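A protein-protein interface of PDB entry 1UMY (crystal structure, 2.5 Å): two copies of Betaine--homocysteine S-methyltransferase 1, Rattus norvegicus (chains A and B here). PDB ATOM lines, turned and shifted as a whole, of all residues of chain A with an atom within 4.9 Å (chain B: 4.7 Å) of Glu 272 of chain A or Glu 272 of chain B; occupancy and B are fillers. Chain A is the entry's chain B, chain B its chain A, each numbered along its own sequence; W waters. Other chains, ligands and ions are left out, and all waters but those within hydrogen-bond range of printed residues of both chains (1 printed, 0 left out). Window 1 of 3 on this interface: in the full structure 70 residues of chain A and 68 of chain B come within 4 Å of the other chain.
The backbone carbonyl oxygen of Lys 35 of chain B sits at hydrogen-bond distance from the backbone NH of Tyr 305 of chain A, at 3.0 Å.
OE2 of Glu 272 of chain B sits at hydrogen-bond distance from OH of Tyr 305 of chain A.
The backbone NH (N) of Tyr 305 of chain B sits at hydrogen-bond distance from the backbone carbonyl oxygen (O) of Lys 35 of chain A, 3.1 Å away.
The side-chain carboxylate (OE2) of Glu 272 of chain A lies within hydrogen-bond range of the side-chain hydroxyl (OH) of Tyr 305 of chain B (2.8 Å).
Among the printed residues, merely in contact across the chains: Phe 269 of chain A with Thr 277 of chain B (3.9 Å), Glu 272 of chain A with Glu 272 of chain B (3.96 Å), Glu 272 of chain A with Val 275 of chain B (3.7 Å), Glu 272 of chain A with Ala 276 of chain B (3.3 Å), Glu 272 of chain A with Thr 277 of chain B (3.2 Å), Pro 273 of chain A with Pro 273 of chain B (3.4 Å), Val 275 of chain A with Glu 272 of chain B (3.6 Å), Ala 276 of chain A with Glu 272 of chain B (3.3 Å), Thr 277 of chain A with Phe 269 of chain B (3.96 Å) and Thr 277 of chain A with Glu 272 of chain B (3.1 Å).
Of the printed residues of chain B, Lys 35 of chain A touches Tyr 305.
Of chain B, only Glu 272 (3.96 Å), Val 275 (3.7 Å), Ala 276 (3.3 Å), Thr 277 (3.2 Å) and Tyr 305 (2.8 Å) come within 4 Å of Glu 272 of chain A.
Of the printed residues of chain B, Val 275 of chain A touches Glu 272 (3.6 Å).
Of the printed residues of chain A, Lys 35 of chain B touches Tyr 305 (3.0 Å).
Of the printed residues of chain A, Thr 277 of chain B touches Phe 269 (3.9 Å) and Glu 272 (3.2 Å).
The nearest residue of chain A that does not touch Glu 272 of chain B is Pro 273 of chain A (4.6 Å).
Printed residues of chain B that touch a printed residue of chain A: Lys 35, Phe 269, Glu 272, Pro 273, Val 275, Ala 276, Thr 277 and Tyr 305.
Of the 12 printed residues of chain A, 8 touch a printed residue of chain B.
Hydrophobic or aromatic side chains of chain A that line the printed part of chain B: Pro 273 and Tyr 305.
Along chain A the printed residues that touch a printed residue of chain B span positions 35 to 305.
Among the printed residues, 14 pairs touch across the chains.
Among the printed residues, no Asp or Glu carboxylate lies within 4 Å of a Lys or Arg side-chain nitrogen of the other chain.
Lys 35 of chain A touches Tyr 305 of chain B, and with the chains exchanged Tyr 305 of chain A touches Lys 35 of chain B.
Glu 272 of chain A touches Thr 277 of chain B, and with the chains exchanged Thr 277 of chain A touches Glu 272 of chain B.
Glu 272 of chain A touches Tyr 305 of chain B, and with the chains exchanged Tyr 305 of chain A touches Glu 272 of chain B.
Pro 273 of chain B touches its own counterpart, Pro 273 of chain A.
11 positions are printed for both chains.
Of the 14 pairs that touch across the chains among the printed residues, 14 have their exchanged pair printed and touching as well.
Water W1 bridges the backbone carbonyl oxygen of Glu 272 of chain B and the backbone carbonyl oxygen of Glu 272 of chain A.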
ATOM      1  N   LYS A  35      18.270 -24.744 -11.579  1.00  0.00           N
ATOM      2  CA  LYS A  35      17.070 -25.526 -11.825  1.00  0.00           C
ATOM      3  C   LYS A  35      17.257 -26.952 -11.353  1.00  0.00           C
ATOM      4  O   LYS A  35      16.282 -27.651 -11.100  1.00  0.00           O
ATOM      5  CB  LYS A  35      16.714 -25.528 -13.311  1.00  0.00           C
ATOM      6  CG  LYS A  35      16.212 -24.213 -13.848  1.00  0.00           C
ATOM      7  CD  LYS A  35      15.933 -24.318 -15.326  1.00  0.00           C
ATOM      8  CE  LYS A  35      15.575 -22.979 -15.907  1.00  0.00           C
ATOM      9  NZ  LYS A  35      16.661 -21.990 -15.693  1.00  0.00           N
ATOM     10  N   TYR A 251      16.767 -16.705 -24.056  1.00  0.00           N
ATOM     11  CA  TYR A 251      15.475 -16.117 -23.751  1.00  0.00           C
ATOM     12  C   TYR A 251      15.098 -15.039 -24.743  1.00  0.00           C
ATOM     13  O   TYR A 251      15.876 -14.136 -25.002  1.00  0.00           O
ATOM     14  CB  TYR A 251      15.499 -15.516 -22.356  1.00  0.00           C
ATOM     15  CG  TYR A 251      15.724 -16.526 -21.274  1.00  0.00           C
ATOM     16  CD1 TYR A 251      14.763 -17.470 -20.986  1.00  0.00           C
ATOM     17  CD2 TYR A 251      16.911 -16.538 -20.532  1.00  0.00           C
ATOM     18  CE1 TYR A 251      14.967 -18.413 -19.982  1.00  0.00           C
ATOM     19  CE2 TYR A 251      17.124 -17.475 -19.534  1.00  0.00           C
ATOM     20  CZ  TYR A 251      16.144 -18.414 -19.265  1.00  0.00           C
ATOM     21  OH  TYR A 251      16.334 -19.374 -18.296  1.00  0.00           O
ATOM     22  N   PHE A 269      12.726 -15.760 -12.044  1.00  0.00           N
ATOM     23  CA  PHE A 269      11.864 -16.907 -11.793  1.00  0.00           C
ATOM     24  C   PHE A 269      10.642 -17.131 -12.690  1.00  0.00           C
ATOM     25  O   PHE A 269       9.870 -18.054 -12.466  1.00  0.00           O
ATOM     26  CB  PHE A 269      11.423 -16.877 -10.336  1.00  0.00           C
ATOM     27  CG  PHE A 269      12.557 -16.950  -9.352  1.00  0.00           C
ATOM     28  CD1 PHE A 269      12.873 -15.862  -8.550  1.00  0.00           C
ATOM     29  CD2 PHE A 269      13.288 -18.120  -9.197  1.00  0.00           C
ATOM     30  CE1 PHE A 269      13.893 -15.938  -7.613  1.00  0.00           C
ATOM     31  CE2 PHE A 269      14.317 -18.209  -8.258  1.00  0.00           C
ATOM     32  CZ  PHE A 269      14.618 -17.118  -7.467  1.00  0.00           C
ATOM     33  N   GLY A 270      10.466 -16.299 -13.703  1.00  0.00           N
ATOM     34  CA  GLY A 270       9.327 -16.466 -14.577  1.00  0.00           C
ATOM     35  C   GLY A 270       9.710 -16.323 -16.032  1.00  0.00           C
ATOM     36  O   GLY A 270       8.901 -15.882 -16.840  1.00  0.00           O
ATOM     37  N   LEU A 271      10.935 -16.709 -16.371  1.00  0.00           N
ATOM     38  CA  LEU A 271      11.431 -16.592 -17.739  1.00  0.00           C
ATOM     39  C   LEU A 271      11.089 -17.794 -18.603  1.00  0.00           C
ATOM     40  O   LEU A 271      11.258 -17.759 -19.811  1.00  0.00           O
ATOM     41  CB  LEU A 271      12.942 -16.412 -17.721  1.00  0.00           C
ATOM     42  CG  LEU A 271      13.472 -15.331 -16.789  1.00  0.00           C
ATOM     43  CD1 LEU A 271      14.965 -15.482 -16.627  1.00  0.00           C
ATOM     44  CD2 LEU A 271      13.116 -13.971 -17.336  1.00  0.00           C
ATOM     45  N   GLU A 272      10.604 -18.850 -17.960  1.00  0.00           N
ATOM     46  CA  GLU A 272      10.237 -20.090 -18.620  1.00  0.00           C
ATOM     47  C   GLU A 272       9.769 -19.967 -20.067  1.00  0.00           C
ATOM     48  O   GLU A 272      10.394 -20.514 -20.971  1.00  0.00           O
ATOM     49  CB  GLU A 272       9.162 -20.814 -17.804  1.00  0.00           C
ATOM     50  CG  GLU A 272       9.668 -21.732 -16.672  1.00  0.00           C
ATOM     51  CD  GLU A 272      10.358 -21.005 -15.508  1.00  0.00           C
ATOM     52  OE1 GLU A 272       9.979 -19.864 -15.173  1.00  0.00           O
ATOM     53  OE2 GLU A 272      11.275 -21.598 -14.909  1.00  0.00           O
ATOM     54  N   PRO A 273       8.670 -19.237 -20.305  1.00  0.00           N
ATOM     55  CA  PRO A 273       8.116 -19.052 -21.642  1.00  0.00           C
ATOM     56  C   PRO A 273       9.018 -18.475 -22.724  1.00  0.00           C
ATOM     57  O   PRO A 273       8.853 -18.786 -23.901  1.00  0.00           O
ATOM     58  CB  PRO A 273       6.895 -18.175 -21.384  1.00  0.00           C
ATOM     59  CG  PRO A 273       7.293 -17.398 -20.223  1.00  0.00           C
ATOM     60  CD  PRO A 273       7.930 -18.415 -19.339  1.00  0.00           C
ATOM     61  N   ARG A 274       9.969 -17.637 -22.339  1.00  0.00           N
ATOM     62  CA  ARG A 274      10.853 -17.020 -23.318  1.00  0.00           C
ATOM     63  C   ARG A 274      11.968 -17.946 -23.792  1.00  0.00           C
ATOM     64  O   ARG A 274      12.679 -17.625 -24.740  1.00  0.00           O
ATOM     65  CB  ARG A 274      11.479 -15.751 -22.740  1.00  0.00           C
ATOM     66  CG  ARG A 274      10.516 -14.700 -22.227  1.00  0.00           C
ATOM     67  CD  ARG A 274      11.204 -13.903 -21.137  1.00  0.00           C
ATOM     68  NE  ARG A 274      10.456 -12.736 -20.688  1.00  0.00           N
ATOM     69  CZ  ARG A 274      10.349 -11.604 -21.373  1.00  0.00           C
ATOM     70  NH1 ARG A 274      10.938 -11.473 -22.548  1.00  0.00           N
ATOM     71  NH2 ARG A 274       9.659 -10.594 -20.875  1.00  0.00           N
ATOM     72  N   VAL A 275      12.128 -19.086 -23.134  1.00  0.00           N
ATOM     73  CA  VAL A 275      13.175 -20.005 -23.507  1.00  0.00           C
ATOM     74  C   VAL A 275      13.097 -20.378 -24.977  1.00  0.00           C
ATOM     75  O   VAL A 275      12.035 -20.697 -25.497  1.00  0.00           O
ATOM     76  CB  VAL A 275      13.119 -21.283 -22.685  1.00  0.00           C
ATOM     77  CG1 VAL A 275      14.230 -22.216 -23.124  1.00  0.00           C
ATOM     78  CG2 VAL A 275      13.239 -20.952 -21.212  1.00  0.00           C
ATOM     79  N   ALA A 276      14.244 -20.349 -25.635  1.00  0.00           N
ATOM     80  CA  ALA A 276      14.326 -20.663 -27.044  1.00  0.00           C
ATOM     81  C   ALA A 276      14.173 -22.160 -27.303  1.00  0.00           C
ATOM     82  O   ALA A 276      14.383 -22.986 -26.414  1.00  0.00           O
ATOM     83  CB  ALA A 276      15.649 -20.179 -27.588  1.00  0.00           C
ATOM     84  N   THR A 277      13.785 -22.504 -28.524  1.00  0.00           N
ATOM     85  CA  THR A 277      13.646 -23.900 -28.895  1.00  0.00           C
ATOM     86  C   THR A 277      14.915 -24.255 -29.630  1.00  0.00           C
ATOM     87  O   THR A 277      15.714 -23.382 -29.954  1.00  0.00           O
ATOM     88  CB  THR A 277      12.487 -24.109 -29.845  1.00  0.00           C
ATOM     89  OG1 THR A 277      12.737 -23.396 -31.059  1.00  0.00           O
ATOM     90  CG2 THR A 277      11.220 -23.629 -29.229  1.00  0.00           C
ATOM     91  N   TYR A 305      20.736 -29.362 -24.984  1.00  0.00           N
ATOM     92  CA  TYR A 305      20.204 -29.465 -26.343  1.00  0.00           C
ATOM     93  C   TYR A 305      20.326 -28.189 -27.155  1.00  0.00           C
ATOM     94  O   TYR A 305      20.277 -28.232 -28.369  1.00  0.00           O
ATOM     95  CB  TYR A 305      18.742 -29.935 -26.340  1.00  0.00           C
ATOM     96  CG  TYR A 305      17.727 -28.925 -25.866  1.00  0.00           C
ATOM     97  CD1 TYR A 305      16.827 -28.336 -26.756  1.00  0.00           C
ATOM     98  CD2 TYR A 305      17.630 -28.591 -24.520  1.00  0.00           C
ATOM     99  CE1 TYR A 305      15.848 -27.443 -26.307  1.00  0.00           C
ATOM    100  CE2 TYR A 305      16.666 -27.712 -24.072  1.00  0.00           C
ATOM    101  CZ  TYR A 305      15.778 -27.143 -24.962  1.00  0.00           C
ATOM    102  OH  TYR A 305      14.817 -26.291 -24.492  1.00  0.00           O
ATOM    103  N   LYS B  35      16.539 -33.693 -23.268  1.00  0.00           N
ATOM    104  CA  LYS B  35      17.141 -32.367 -23.346  1.00  0.00           C
ATOM    105  C   LYS B  35      18.597 -32.397 -22.944  1.00  0.00           C
ATOM    106  O   LYS B  35      19.363 -31.502 -23.307  1.00  0.00           O
ATOM    107  CB  LYS B  35      16.398 -31.374 -22.459  1.00  0.00           C
ATOM    108  CG  LYS B  35      15.014 -30.983 -22.957  1.00  0.00           C
ATOM    109  CD  LYS B  35      14.350 -30.067 -21.955  1.00  0.00           C
ATOM    110  CE  LYS B  35      12.920 -29.784 -22.333  1.00  0.00           C
ATOM    111  NZ  LYS B  35      12.133 -31.043 -22.402  1.00  0.00           N
ATOM    112  N   PHE B 269       8.844 -30.819 -29.955  1.00  0.00           N
ATOM    113  CA  PHE B 269       9.987 -29.925 -30.063  1.00  0.00           C
ATOM    114  C   PHE B 269       9.772 -28.413 -29.942  1.00  0.00           C
ATOM    115  O   PHE B 269      10.710 -27.642 -30.096  1.00  0.00           O
ATOM    116  CB  PHE B 269      10.720 -30.226 -31.362  1.00  0.00           C
ATOM    117  CG  PHE B 269      11.237 -31.631 -31.449  1.00  0.00           C
ATOM    118  CD1 PHE B 269      10.696 -32.522 -32.350  1.00  0.00           C
ATOM    119  CD2 PHE B 269      12.283 -32.053 -30.645  1.00  0.00           C
ATOM    120  CE1 PHE B 269      11.192 -33.815 -32.459  1.00  0.00           C
ATOM    121  CE2 PHE B 269      12.786 -33.339 -30.742  1.00  0.00           C
ATOM    122  CZ  PHE B 269      12.242 -34.225 -31.652  1.00  0.00           C
ATOM    123  N   GLY B 270       8.548 -27.989 -29.667  1.00  0.00           N
ATOM    124  CA  GLY B 270       8.290 -26.572 -29.533  1.00  0.00           C
ATOM    125  C   GLY B 270       7.412 -26.273 -28.337  1.00  0.00           C
ATOM    126  O   GLY B 270       6.648 -25.330 -28.359  1.00  0.00           O
ATOM    127  N   LEU B 271       7.531 -27.071 -27.285  1.00  0.00           N
ATOM    128  CA  LEU B 271       6.706 -26.893 -26.096  1.00  0.00           C
ATOM    129  C   LEU B 271       7.291 -25.905 -25.095  1.00  0.00           C
ATOM    130  O   LEU B 271       6.620 -25.476 -24.165  1.00  0.00           O
ATOM    131  CB  LEU B 271       6.505 -28.243 -25.417  1.00  0.00           C
ATOM    132  CG  LEU B 271       6.028 -29.380 -26.320  1.00  0.00           C
ATOM    133  CD1 LEU B 271       6.184 -30.706 -25.610  1.00  0.00           C
ATOM    134  CD2 LEU B 271       4.590 -29.141 -26.718  1.00  0.00           C
ATOM    135  N   GLU B 272       8.553 -25.557 -25.307  1.00  0.00           N
ATOM    136  CA  GLU B 272       9.288 -24.644 -24.450  1.00  0.00           C
ATOM    137  C   GLU B 272       8.448 -23.603 -23.704  1.00  0.00           C
ATOM    138  O   GLU B 272       8.400 -23.591 -22.477  1.00  0.00           O
ATOM    139  CB  GLU B 272      10.372 -23.929 -25.269  1.00  0.00           C
ATOM    140  CG  GLU B 272      11.712 -24.653 -25.423  1.00  0.00           C
ATOM    141  CD  GLU B 272      11.653 -25.938 -26.230  1.00  0.00           C
ATOM    142  OE1 GLU B 272      10.885 -26.016 -27.213  1.00  0.00           O
ATOM    143  OE2 GLU B 272      12.408 -26.865 -25.881  1.00  0.00           O
ATOM    144  N   PRO B 273       7.763 -22.724 -24.439  1.00  0.00           N
ATOM    145  CA  PRO B 273       6.941 -21.676 -23.838  1.00  0.00           C
ATOM    146  C   PRO B 273       5.860 -22.079 -22.857  1.00  0.00           C
ATOM    147  O   PRO B 273       5.537 -21.315 -21.951  1.00  0.00           O
ATOM    148  CB  PRO B 273       6.371 -20.952 -25.058  1.00  0.00           C
ATOM    149  CG  PRO B 273       6.276 -22.018 -26.066  1.00  0.00           C
ATOM    150  CD  PRO B 273       7.580 -22.743 -25.900  1.00  0.00           C
ATOM    151  N   ARG B 274       5.298 -23.267 -23.030  1.00  0.00           N
ATOM    152  CA  ARG B 274       4.226 -23.725 -22.155  1.00  0.00           C
ATOM    153  C   ARG B 274       4.725 -24.244 -20.822  1.00  0.00           C
ATOM    154  O   ARG B 274       3.936 -24.503 -19.927  1.00  0.00           O
ATOM    155  CB  ARG B 274       3.418 -24.829 -22.837  1.00  0.00           C
ATOM    156  CG  ARG B 274       2.787 -24.471 -24.168  1.00  0.00           C
ATOM    157  CD  ARG B 274       2.635 -25.743 -24.984  1.00  0.00           C
ATOM    158  NE  ARG B 274       1.904 -25.568 -26.235  1.00  0.00           N
ATOM    159  CZ  ARG B 274       0.588 -25.429 -26.325  1.00  0.00           C
ATOM    160  NH1 ARG B 274      -0.171 -25.435 -25.242  1.00  0.00           N
ATOM    161  NH2 ARG B 274       0.032 -25.313 -27.513  1.00  0.00           N
ATOM    162  N   VAL B 275       6.033 -24.407 -20.685  1.00  0.00           N
ATOM    163  CA  VAL B 275       6.579 -24.931 -19.449  1.00  0.00           C
ATOM    164  C   VAL B 275       6.138 -24.101 -18.271  1.00  0.00           C
ATOM    165  O   VAL B 275       6.162 -22.882 -18.316  1.00  0.00           O
ATOM    166  CB  VAL B 275       8.110 -24.968 -19.482  1.00  0.00           C
ATOM    167  CG1 VAL B 275       8.641 -25.526 -18.181  1.00  0.00           C
ATOM    168  CG2 VAL B 275       8.577 -25.817 -20.636  1.00  0.00           C
ATOM    169  N   ALA B 276       5.747 -24.782 -17.207  1.00  0.00           N
ATOM    170  CA  ALA B 276       5.291 -24.133 -15.992  1.00  0.00           C
ATOM    171  C   ALA B 276       6.446 -23.535 -15.219  1.00  0.00           C
ATOM    172  O   ALA B 276       7.592 -23.928 -15.401  1.00  0.00           O
ATOM    173  CB  ALA B 276       4.559 -25.135 -15.111  1.00  0.00           C
ATOM    174  N   THR B 277       6.137 -22.560 -14.373  1.00  0.00           N
ATOM    175  CA  THR B 277       7.144 -21.942 -13.531  1.00  0.00           C
ATOM    176  C   THR B 277       7.015 -22.610 -12.175  1.00  0.00           C
ATOM    177  O   THR B 277       6.072 -23.350 -11.939  1.00  0.00           O
ATOM    178  CB  THR B 277       6.897 -20.453 -13.330  1.00  0.00           C
ATOM    179  OG1 THR B 277       5.666 -20.264 -12.632  1.00  0.00           O
ATOM    180  CG2 THR B 277       6.865 -19.755 -14.629  1.00  0.00           C
ATOM    181  N   TYR B 305      13.500 -28.555 -10.204  1.00  0.00           N
ATOM    182  CA  TYR B 305      12.923 -27.443  -9.448  1.00  0.00           C
ATOM    183  C   TYR B 305      11.413 -27.475  -9.368  1.00  0.00           C
ATOM    184  O   TYR B 305      10.836 -26.883  -8.468  1.00  0.00           O
ATOM    185  CB  TYR B 305      13.378 -26.086  -9.992  1.00  0.00           C
ATOM    186  CG  TYR B 305      12.794 -25.675 -11.325  1.00  0.00           C
ATOM    187  CD1 TYR B 305      11.887 -24.618 -11.418  1.00  0.00           C
ATOM    188  CD2 TYR B 305      13.195 -26.297 -12.495  1.00  0.00           C
ATOM    189  CE1 TYR B 305      11.404 -24.197 -12.647  1.00  0.00           C
ATOM    190  CE2 TYR B 305      12.726 -25.887 -13.715  1.00  0.00           C
ATOM    191  CZ  TYR B 305      11.835 -24.839 -13.795  1.00  0.00           C
ATOM    192  OH  TYR B 305      11.406 -24.441 -15.037  1.00  0.00           O
HETATM  193  O   HOH W   1      10.432 -23.391 -20.985  1.00  0.00           O
